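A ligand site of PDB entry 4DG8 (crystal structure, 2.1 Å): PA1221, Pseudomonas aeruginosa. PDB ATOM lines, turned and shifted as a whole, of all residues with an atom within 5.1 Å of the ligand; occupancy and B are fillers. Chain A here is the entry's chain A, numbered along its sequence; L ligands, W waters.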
ATOM      1  N   ASP A 216      22.439  -9.302  23.981  1.00  0.00           N
ATOM      2  CA  ASP A 216      21.472  -8.852  22.972  1.00  0.00           C
ATOM      3  C   ASP A 216      20.037  -9.295  23.286  1.00  0.00           C
ATOM      4  O   ASP A 216      19.128  -9.007  22.496  1.00  0.00           O
ATOM      5  CB  ASP A 216      21.880  -9.184  21.514  1.00  0.00           C
ATOM      6  CG  ASP A 216      21.846 -10.667  21.210  1.00  0.00           C
ATOM      7  OD1 ASP A 216      22.146 -11.035  20.049  1.00  0.00           O
ATOM      8  OD2 ASP A 216      21.522 -11.468  22.108  1.00  0.00           O
ATOM      9  N   THR A 283      11.951 -17.476  26.560  1.00  0.00           N
ATOM     10  CA  THR A 283      13.075 -18.051  27.278  1.00  0.00           C
ATOM     11  C   THR A 283      13.985 -18.766  26.280  1.00  0.00           C
ATOM     12  O   THR A 283      13.625 -18.895  25.103  1.00  0.00           O
ATOM     13  CB  THR A 283      12.610 -19.023  28.384  1.00  0.00           C
ATOM     14  OG1 THR A 283      13.759 -19.478  29.110  1.00  0.00           O
ATOM     15  CG2 THR A 283      11.888 -20.231  27.765  1.00  0.00           C
ATOM     16  N   GLY A 284      15.170 -19.157  26.713  1.00  0.00           N
ATOM     17  CA  GLY A 284      16.150 -19.714  25.795  1.00  0.00           C
ATOM     18  C   GLY A 284      17.571 -19.430  26.239  1.00  0.00           C
ATOM     19  O   GLY A 284      17.836 -19.259  27.433  1.00  0.00           O
ATOM     20  N   GLY A 285      18.490 -19.381  25.275  1.00  0.00           N
ATOM     21  CA  GLY A 285      19.875 -19.098  25.596  1.00  0.00           C
ATOM     22  C   GLY A 285      20.645 -20.364  25.929  1.00  0.00           C
ATOM     23  O   GLY A 285      21.858 -20.412  25.776  1.00  0.00           O
ATOM     24  N   ASP A 286      19.915 -21.378  26.370  1.00  0.00           N
ATOM     25  CA  ASP A 286      20.429 -22.732  26.571  1.00  0.00           C
ATOM     26  C   ASP A 286      19.305 -23.693  26.233  1.00  0.00           C
ATOM     27  O   ASP A 286      18.159 -23.273  26.060  1.00  0.00           O
ATOM     28  CB  ASP A 286      20.853 -22.976  28.022  1.00  0.00           C
ATOM     29  CG  ASP A 286      22.291 -22.618  28.277  1.00  0.00           C
ATOM     30  OD1 ASP A 286      23.190 -23.281  27.707  1.00  0.00           O
ATOM     31  OD2 ASP A 286      22.511 -21.675  29.070  1.00  0.00           O
ATOM     32  N   ILE A 287      19.645 -24.975  26.140  1.00  0.00           N
ATOM     33  CA  ILE A 287      18.649 -26.027  25.997  1.00  0.00           C
ATOM     34  C   ILE A 287      17.625 -25.903  27.138  1.00  0.00           C
ATOM     35  O   ILE A 287      17.976 -25.902  28.321  1.00  0.00           O
ATOM     36  CB  ILE A 287      19.335 -27.419  26.031  1.00  0.00           C
ATOM     37  CG1 ILE A 287      20.127 -27.644  24.745  1.00  0.00           C
ATOM     38  CG2 ILE A 287      18.326 -28.594  26.250  1.00  0.00           C
ATOM     39  CD1 ILE A 287      21.105 -28.856  24.837  1.00  0.00           C
ATOM     40  N   LEU A 288      16.363 -25.810  26.754  1.00  0.00           N
ATOM     41  CA  LEU A 288      15.303 -25.679  27.741  1.00  0.00           C
ATOM     42  C   LEU A 288      15.116 -27.003  28.477  1.00  0.00           C
ATOM     43  O   LEU A 288      15.274 -28.093  27.900  1.00  0.00           O
ATOM     44  CB  LEU A 288      13.994 -25.229  27.090  1.00  0.00           C
ATOM     45  CG  LEU A 288      13.943 -23.928  26.292  1.00  0.00           C
ATOM     46  CD1 LEU A 288      12.476 -23.614  25.987  1.00  0.00           C
ATOM     47  CD2 LEU A 288      14.593 -22.768  27.055  1.00  0.00           C
ATOM     48  N   ASN A 307      10.216 -20.457  22.916  1.00  0.00           N
ATOM     49  CA  ASN A 307      11.618 -20.856  22.987  1.00  0.00           C
ATOM     50  C   ASN A 307      12.332 -20.064  21.887  1.00  0.00           C
ATOM     51  O   ASN A 307      12.075 -20.284  20.712  1.00  0.00           O
ATOM     52  CB  ASN A 307      11.752 -22.368  22.743  1.00  0.00           C
ATOM     53  CG  ASN A 307      13.187 -22.893  22.891  1.00  0.00           C
ATOM     54  OD1 ASN A 307      14.100 -22.150  23.269  1.00  0.00           O
ATOM     55  ND2 ASN A 307      13.392 -24.190  22.613  1.00  0.00           N
ATOM     56  N   GLY A 308      13.128 -19.068  22.275  1.00  0.00           N
ATOM     57  CA  GLY A 308      13.945 -18.355  21.317  1.00  0.00           C
ATOM     58  C   GLY A 308      15.368 -18.895  21.225  1.00  0.00           C
ATOM     59  O   GLY A 308      16.042 -19.060  22.247  1.00  0.00           O
ATOM     60  N   TYR A 309      15.869 -19.017  20.001  1.00  0.00           N
ATOM     61  CA  TYR A 309      17.216 -19.520  19.761  1.00  0.00           C
ATOM     62  C   TYR A 309      17.910 -18.585  18.787  1.00  0.00           C
ATOM     63  O   TYR A 309      17.297 -18.148  17.822  1.00  0.00           O
ATOM     64  CB  TYR A 309      17.196 -20.924  19.140  1.00  0.00           C
ATOM     65  CG  TYR A 309      18.412 -21.142  18.258  1.00  0.00           C
ATOM     66  CD1 TYR A 309      19.621 -21.544  18.812  1.00  0.00           C
ATOM     67  CD2 TYR A 309      18.377 -20.884  16.886  1.00  0.00           C
ATOM     68  CE1 TYR A 309      20.745 -21.723  18.038  1.00  0.00           C
ATOM     69  CE2 TYR A 309      19.498 -21.051  16.094  1.00  0.00           C
ATOM     70  CZ  TYR A 309      20.694 -21.467  16.684  1.00  0.00           C
ATOM     71  OH  TYR A 309      21.842 -21.640  15.938  1.00  0.00           O
ATOM     72  N   GLY A 310      19.170 -18.251  19.055  1.00  0.00           N
ATOM     73  CA  GLY A 310      19.976 -17.626  18.028  1.00  0.00           C
ATOM     74  C   GLY A 310      21.296 -17.124  18.552  1.00  0.00           C
ATOM     75  O   GLY A 310      21.429 -16.870  19.767  1.00  0.00           O
ATOM     76  N   PRO A 311      22.294 -16.949  17.661  1.00  0.00           N
ATOM     77  CA  PRO A 311      23.519 -16.323  18.172  1.00  0.00           C
ATOM     78  C   PRO A 311      23.513 -14.814  17.968  1.00  0.00           C
ATOM     79  O   PRO A 311      22.673 -14.269  17.240  1.00  0.00           O
ATOM     80  CB  PRO A 311      24.601 -16.991  17.320  1.00  0.00           C
ATOM     81  CG  PRO A 311      23.912 -17.249  15.991  1.00  0.00           C
ATOM     82  CD  PRO A 311      22.446 -17.477  16.294  1.00  0.00           C
ATOM     83  N   THR A 312      24.505 -14.139  18.538  1.00  0.00           N
ATOM     84  CA  THR A 312      24.566 -12.684  18.504  1.00  0.00           C
ATOM     85  C   THR A 312      24.838 -12.154  17.080  1.00  0.00           C
ATOM     86  O   THR A 312      24.341 -11.089  16.698  1.00  0.00           O
ATOM     87  CB  THR A 312      25.643 -12.176  19.510  1.00  0.00           C
ATOM     88  OG1 THR A 312      25.298 -12.627  20.831  1.00  0.00           O
ATOM     89  CG2 THR A 312      25.771 -10.644  19.496  1.00  0.00           C
ATOM     90  N   GLU A 313      25.618 -12.917  16.308  1.00  0.00           N
ATOM     91  CA  GLU A 313      25.916 -12.599  14.908  1.00  0.00           C
ATOM     92  C   GLU A 313      24.677 -12.498  14.013  1.00  0.00           C
ATOM     93  O   GLU A 313      24.741 -11.972  12.882  1.00  0.00           O
ATOM     94  CB  GLU A 313      26.859 -13.677  14.323  1.00  0.00           C
ATOM     95  CG  GLU A 313      28.277 -13.687  14.886  1.00  0.00           C
ATOM     96  CD  GLU A 313      28.403 -14.406  16.242  1.00  0.00           C
ATOM     97  OE1 GLU A 313      27.356 -14.720  16.890  1.00  0.00           O
ATOM     98  OE2 GLU A 313      29.561 -14.650  16.655  1.00  0.00           O
ATOM     99  N   ILE A 335      13.073 -25.598  18.741  1.00  0.00           N
ATOM    100  CA  ILE A 335      13.458 -24.194  18.592  1.00  0.00           C
ATOM    101  C   ILE A 335      12.714 -23.590  17.410  1.00  0.00           C
ATOM    102  O   ILE A 335      12.856 -22.419  17.093  1.00  0.00           O
ATOM    103  CB  ILE A 335      14.994 -23.977  18.468  1.00  0.00           C
ATOM    104  CG1 ILE A 335      15.565 -24.725  17.253  1.00  0.00           C
ATOM    105  CG2 ILE A 335      15.693 -24.390  19.774  1.00  0.00           C
ATOM    106  CD1 ILE A 335      17.093 -24.550  17.067  1.00  0.00           C
ATOM    107  N   THR A 400      26.483 -21.099  12.213  1.00  0.00           N
ATOM    108  CA  THR A 400      26.374 -20.874  13.649  1.00  0.00           C
ATOM    109  C   THR A 400      27.296 -21.733  14.518  1.00  0.00           C
ATOM    110  O   THR A 400      27.602 -21.366  15.666  1.00  0.00           O
ATOM    111  CB  THR A 400      24.932 -21.140  14.130  1.00  0.00           C
ATOM    112  OG1 THR A 400      24.574 -22.470  13.779  1.00  0.00           O
ATOM    113  CG2 THR A 400      23.939 -20.156  13.508  1.00  0.00           C
ATOM    114  N   ASP A 402      26.057 -24.394  15.505  1.00  0.00           N
ATOM    115  CA  ASP A 402      25.027 -25.145  16.215  1.00  0.00           C
ATOM    116  C   ASP A 402      24.521 -26.332  15.386  1.00  0.00           C
ATOM    117  O   ASP A 402      24.291 -26.214  14.171  1.00  0.00           O
ATOM    118  CB  ASP A 402      23.862 -24.232  16.626  1.00  0.00           C
ATOM    119  CG  ASP A 402      24.262 -23.228  17.683  1.00  0.00           C
ATOM    120  OD1 ASP A 402      24.966 -23.600  18.654  1.00  0.00           O
ATOM    121  OD2 ASP A 402      23.857 -22.057  17.561  1.00  0.00           O
ATOM    122  N   PHE A 414      17.134 -28.577  18.536  1.00  0.00           N
ATOM    123  CA  PHE A 414      18.524 -28.268  18.854  1.00  0.00           C
ATOM    124  C   PHE A 414      19.269 -29.483  19.424  1.00  0.00           C
ATOM    125  O   PHE A 414      18.798 -30.177  20.329  1.00  0.00           O
ATOM    126  CB  PHE A 414      18.591 -27.099  19.830  1.00  0.00           C
ATOM    127  CG  PHE A 414      19.986 -26.659  20.155  1.00  0.00           C
ATOM    128  CD1 PHE A 414      20.587 -25.640  19.415  1.00  0.00           C
ATOM    129  CD2 PHE A 414      20.693 -27.240  21.196  1.00  0.00           C
ATOM    130  CE1 PHE A 414      21.874 -25.221  19.705  1.00  0.00           C
ATOM    131  CE2 PHE A 414      21.976 -26.827  21.493  1.00  0.00           C
ATOM    132  CZ  PHE A 414      22.575 -25.822  20.755  1.00  0.00           C
ATOM    133  N   ARG A 417      26.777 -28.498  20.296  1.00  0.00           N
ATOM    134  CA  ARG A 417      27.961 -28.044  19.573  1.00  0.00           C
ATOM    135  C   ARG A 417      29.073 -29.087  19.582  1.00  0.00           C
ATOM    136  O   ARG A 417      29.130 -29.945  20.450  1.00  0.00           O
ATOM    137  CB  ARG A 417      28.489 -26.717  20.121  1.00  0.00           C
ATOM    138  CG  ARG A 417      27.469 -25.570  20.030  1.00  0.00           C
ATOM    139  CD  ARG A 417      28.021 -24.302  20.612  1.00  0.00           C
ATOM    140  NE  ARG A 417      29.141 -23.788  19.814  1.00  0.00           N
ATOM    141  CZ  ARG A 417      29.000 -23.077  18.709  1.00  0.00           C
ATOM    142  NH1 ARG A 417      27.777 -22.783  18.254  1.00  0.00           N
ATOM    143  NH2 ARG A 417      30.076 -22.654  18.050  1.00  0.00           N
ATOM    144  N   GLN A 421      32.655 -24.579  23.180  1.00  0.00           N
ATOM    145  CA  GLN A 421      31.971 -23.365  23.606  1.00  0.00           C
ATOM    146  C   GLN A 421      30.849 -23.655  24.608  1.00  0.00           C
ATOM    147  O   GLN A 421      29.974 -24.477  24.345  1.00  0.00           O
ATOM    148  CB  GLN A 421      31.423 -22.617  22.400  1.00  0.00           C
ATOM    149  CG  GLN A 421      30.488 -21.478  22.746  1.00  0.00           C
ATOM    150  CD  GLN A 421      30.017 -20.720  21.501  1.00  0.00           C
ATOM    151  OE1 GLN A 421      30.821 -20.142  20.765  1.00  0.00           O
ATOM    152  NE2 GLN A 421      28.705 -20.736  21.264  1.00  0.00           N
ATOM    153  N   LYS A 423      27.944 -21.863  27.609  1.00  0.00           N
ATOM    154  CA  LYS A 423      27.253 -20.642  28.023  1.00  0.00           C
ATOM    155  C   LYS A 423      27.432 -20.402  29.524  1.00  0.00           C
ATOM    156  O   LYS A 423      26.984 -21.214  30.337  1.00  0.00           O
ATOM    157  CB  LYS A 423      25.761 -20.700  27.668  1.00  0.00           C
ATOM    158  CG  LYS A 423      25.428 -20.755  26.164  1.00  0.00           C
ATOM    159  CD  LYS A 423      25.754 -19.429  25.460  1.00  0.00           C
ATOM    160  CE  LYS A 423      24.795 -18.278  25.856  1.00  0.00           C
ATOM    161  NZ  LYS A 423      23.485 -18.286  25.140  1.00  0.00           N
ATOM    162  N   GLY A 426      24.969 -16.111  30.667  1.00  0.00           N
ATOM    163  CA  GLY A 426      24.587 -15.243  29.555  1.00  0.00           C
ATOM    164  C   GLY A 426      25.650 -15.051  28.494  1.00  0.00           C
ATOM    165  O   GLY A 426      25.344 -14.615  27.393  1.00  0.00           O
ATOM    166  N   TYR A 427      26.896 -15.388  28.822  1.00  0.00           N
ATOM    167  CA  TYR A 427      28.013 -15.219  27.885  1.00  0.00           C
ATOM    168  C   TYR A 427      28.465 -16.535  27.248  1.00  0.00           C
ATOM    169  O   TYR A 427      28.580 -17.559  27.925  1.00  0.00           O
ATOM    170  CB  TYR A 427      29.225 -14.615  28.598  1.00  0.00           C
ATOM    171  CG  TYR A 427      29.010 -13.239  29.180  1.00  0.00           C
ATOM    172  CD1 TYR A 427      28.859 -12.142  28.345  1.00  0.00           C
ATOM    173  CD2 TYR A 427      28.981 -13.036  30.553  1.00  0.00           C
ATOM    174  CE1 TYR A 427      28.690 -10.869  28.869  1.00  0.00           C
ATOM    175  CE2 TYR A 427      28.805 -11.766  31.098  1.00  0.00           C
ATOM    176  CZ  TYR A 427      28.669 -10.690  30.241  1.00  0.00           C
ATOM    177  OH  TYR A 427      28.491  -9.423  30.757  1.00  0.00           O
ATOM    178  N   ARG A 428      28.735 -16.510  25.946  1.00  0.00           N
ATOM    179  CA  ARG A 428      29.492 -17.602  25.340  1.00  0.00           C
ATOM    180  C   ARG A 428      30.964 -17.534  25.800  1.00  0.00           C
ATOM    181  O   ARG A 428      31.562 -16.455  25.944  1.00  0.00           O
ATOM    182  CB  ARG A 428      29.424 -17.547  23.817  1.00  0.00           C
ATOM    183  CG  ARG A 428      28.067 -17.882  23.245  1.00  0.00           C
ATOM    184  CD  ARG A 428      28.036 -17.608  21.730  1.00  0.00           C
ATOM    185  NE  ARG A 428      28.221 -16.190  21.417  1.00  0.00           N
ATOM    186  CZ  ARG A 428      28.079 -15.668  20.198  1.00  0.00           C
ATOM    187  NH1 ARG A 428      27.770 -16.459  19.180  1.00  0.00           N
ATOM    188  NH2 ARG A 428      28.263 -14.372  20.004  1.00  0.00           N
HETATM  189  P1  LIG L   1      24.519 -15.671  22.445  1.00  0.00           P
HETATM  190  O1  LIG L   1      25.320 -15.163  23.626  1.00  0.00           O
HETATM  191  O2  LIG L   1      23.052 -15.253  22.323  1.00  0.00           O
HETATM  192  O3  LIG L   1      25.287 -15.285  21.197  1.00  0.00           O
HETATM  193  O4  LIG L   1      24.609 -17.253  22.381  1.00  0.00           O
HETATM  194  C1  LIG L   1      24.160 -17.955  21.240  1.00  0.00           C
HETATM  195  C2  LIG L   1      24.293 -19.447  21.417  1.00  0.00           C
HETATM  196  O5  LIG L   1      23.562 -19.870  22.601  1.00  0.00           O
HETATM  197  C3  LIG L   1      23.715 -20.292  20.288  1.00  0.00           C
HETATM  198  O6  LIG L   1      24.594 -20.392  19.183  1.00  0.00           O
HETATM  199  C4  LIG L   1      23.445 -21.621  20.985  1.00  0.00           C
HETATM  200  O7  LIG L   1      24.648 -22.365  21.137  1.00  0.00           O
HETATM  201  C5  LIG L   1      22.984 -21.145  22.372  1.00  0.00           C
HETATM  202  N1  LIG L   1      21.516 -21.024  22.460  1.00  0.00           N
HETATM  203  C6  LIG L   1      20.830 -19.854  22.393  1.00  0.00           C
HETATM  204  N2  LIG L   1      19.499 -20.051  22.512  1.00  0.00           N
HETATM  205  C7  LIG L   1      19.281 -21.364  22.639  1.00  0.00           C
HETATM  206  C8  LIG L   1      18.099 -22.249  22.793  1.00  0.00           C
HETATM  207  N3  LIG L   1      16.848 -21.740  22.828  1.00  0.00           N
HETATM  208  N4  LIG L   1      18.304 -23.581  22.910  1.00  0.00           N
HETATM  209  C9  LIG L   1      19.551 -24.096  22.883  1.00  0.00           C
HETATM  210  N5  LIG L   1      20.668 -23.350  22.743  1.00  0.00           N
HETATM  211  C10 LIG L   1      20.615 -22.010  22.616  1.00  0.00           C
HETATM  212  O   HOH W   1      27.308 -19.482  19.140  1.00  0.00           O
HETATM  213  O   HOH W   2      26.752 -21.602  22.822  1.00  0.00           O
HETATM  214  O   HOH W   3      28.037 -14.578  23.973  1.00  0.00           O
HETATM  215  O   HOH W   4      24.574 -13.443  25.322  1.00  0.00           O
HETATM  216  O   HOH W   5      23.093 -24.512  24.045  1.00  0.00           O
HETATM  217  O   HOH W   6      15.973 -25.294  23.747  1.00  0.00           O
HETATM  218  O   HOH W   7      21.765 -13.885  20.434  1.00  0.00           O
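The backbone carbonyl oxygen (O) of Gly 308 is in hydrogen-bond range of a nitrogen (N3) of the ligand (2.9 Å).
The side-chain hydroxyl (OG1) of Thr 312 sits at hydrogen-bond distance from an oxygen (O3) of the ligand, 2.7 Å away.
An oxygen (O3) of the ligand is in salt-bridge range of the guanidinium group (NE) of Arg 428, 3.1 Å away.
The backbone NH (N) of Gly 285 is in hydrogen-bond range of a nitrogen (N2) of the ligand.
OD2 of Asp 402 is in hydrogen-bond range of O6 of the ligand.
The side-chain amide oxygen (OD1) of Asn 307 sits at hydrogen-bond distance from a nitrogen (N3) of the ligand, 2.8 Å away.
The backbone NH of Thr 312 sits at hydrogen-bond distance from an oxygen (O3) of the ligand (3.0 Å).
The side-chain amino group of Lys 423 is in salt-bridge range of an oxygen (O1) of the ligand (3.9 Å).
OD1 of Asp 402 lies within salt-bridge range of NH1 of Arg 417, 3.0 Å away.
OH of Tyr 309 is in hydrogen-bond range of OD2 of Asp 402 (2.6 Å).
The guanidinium group of Arg 417 sits close to the side-chain amide nitrogen of Gln 421, at 3.4 Å.
NH1 of Arg 428 is in salt-bridge range of OE1 of Glu 313.
The backbone NH (N) of Asp 402 sits at hydrogen-bond distance from the side-chain hydroxyl (OG1) of Thr 400.
N of Gly 308 is in hydrogen-bond range of O of Thr 283, at 2.9 Å.
The side-chain amino group (NZ) of Lys 423 lies within hydrogen-bond range of the backbone carbonyl oxygen (O) of Gly 285 (2.8 Å).
The guanidinium group (NH1) of Arg 417 lies within hydrogen-bond range of the backbone carbonyl oxygen (O) of Thr 400 (3.0 Å).
A nitrogen (N4) of the ligand lies close to the backbone carbonyl oxygen (O) of Asp 286 (3.2 Å).
The backbone carbonyl oxygen (O) of Gly 310 lies close to an oxygen (O2) of the ligand (3.4 Å).
CA of Gly 284 touches N3 of the ligand (3.7 Å).
N of Ile 287 touches C9 of the ligand, at 3.4 Å.
Tyr 309 touches the ligand (CA to N2, 3.6 Å).
Pro 311 touches the ligand.
Phe 414 touches the ligand.
Arg 417 touches the ligand (CD to O7, 3.9 Å).
Gly 426 touches the ligand.
Hydrophobic or aromatic side chains within 4 Å of the ligand: Tyr 309, Pro 311 and Phe 414.
Of the 24 residues printed, 16 come within 4 Å of the ligand.
Water W4 bridges O of Gly 426 (2.5 Å) and O1 of the ligand (2.5 Å).
Water W3 lies within hydrogen-bond range of O1 of the ligand (2.8 Å) and N of Arg 428 (2.8 Å).
Water W2 bridges the side-chain amide nitrogen (NE2) of Gln 421 and an oxygen (O7) of the ligand.
Water W6 lies within hydrogen-bond range of N4 of the ligand (3.0 Å), ND2 of Asn 307 (3.0 Å) and N of Leu 288 (3.1 Å).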
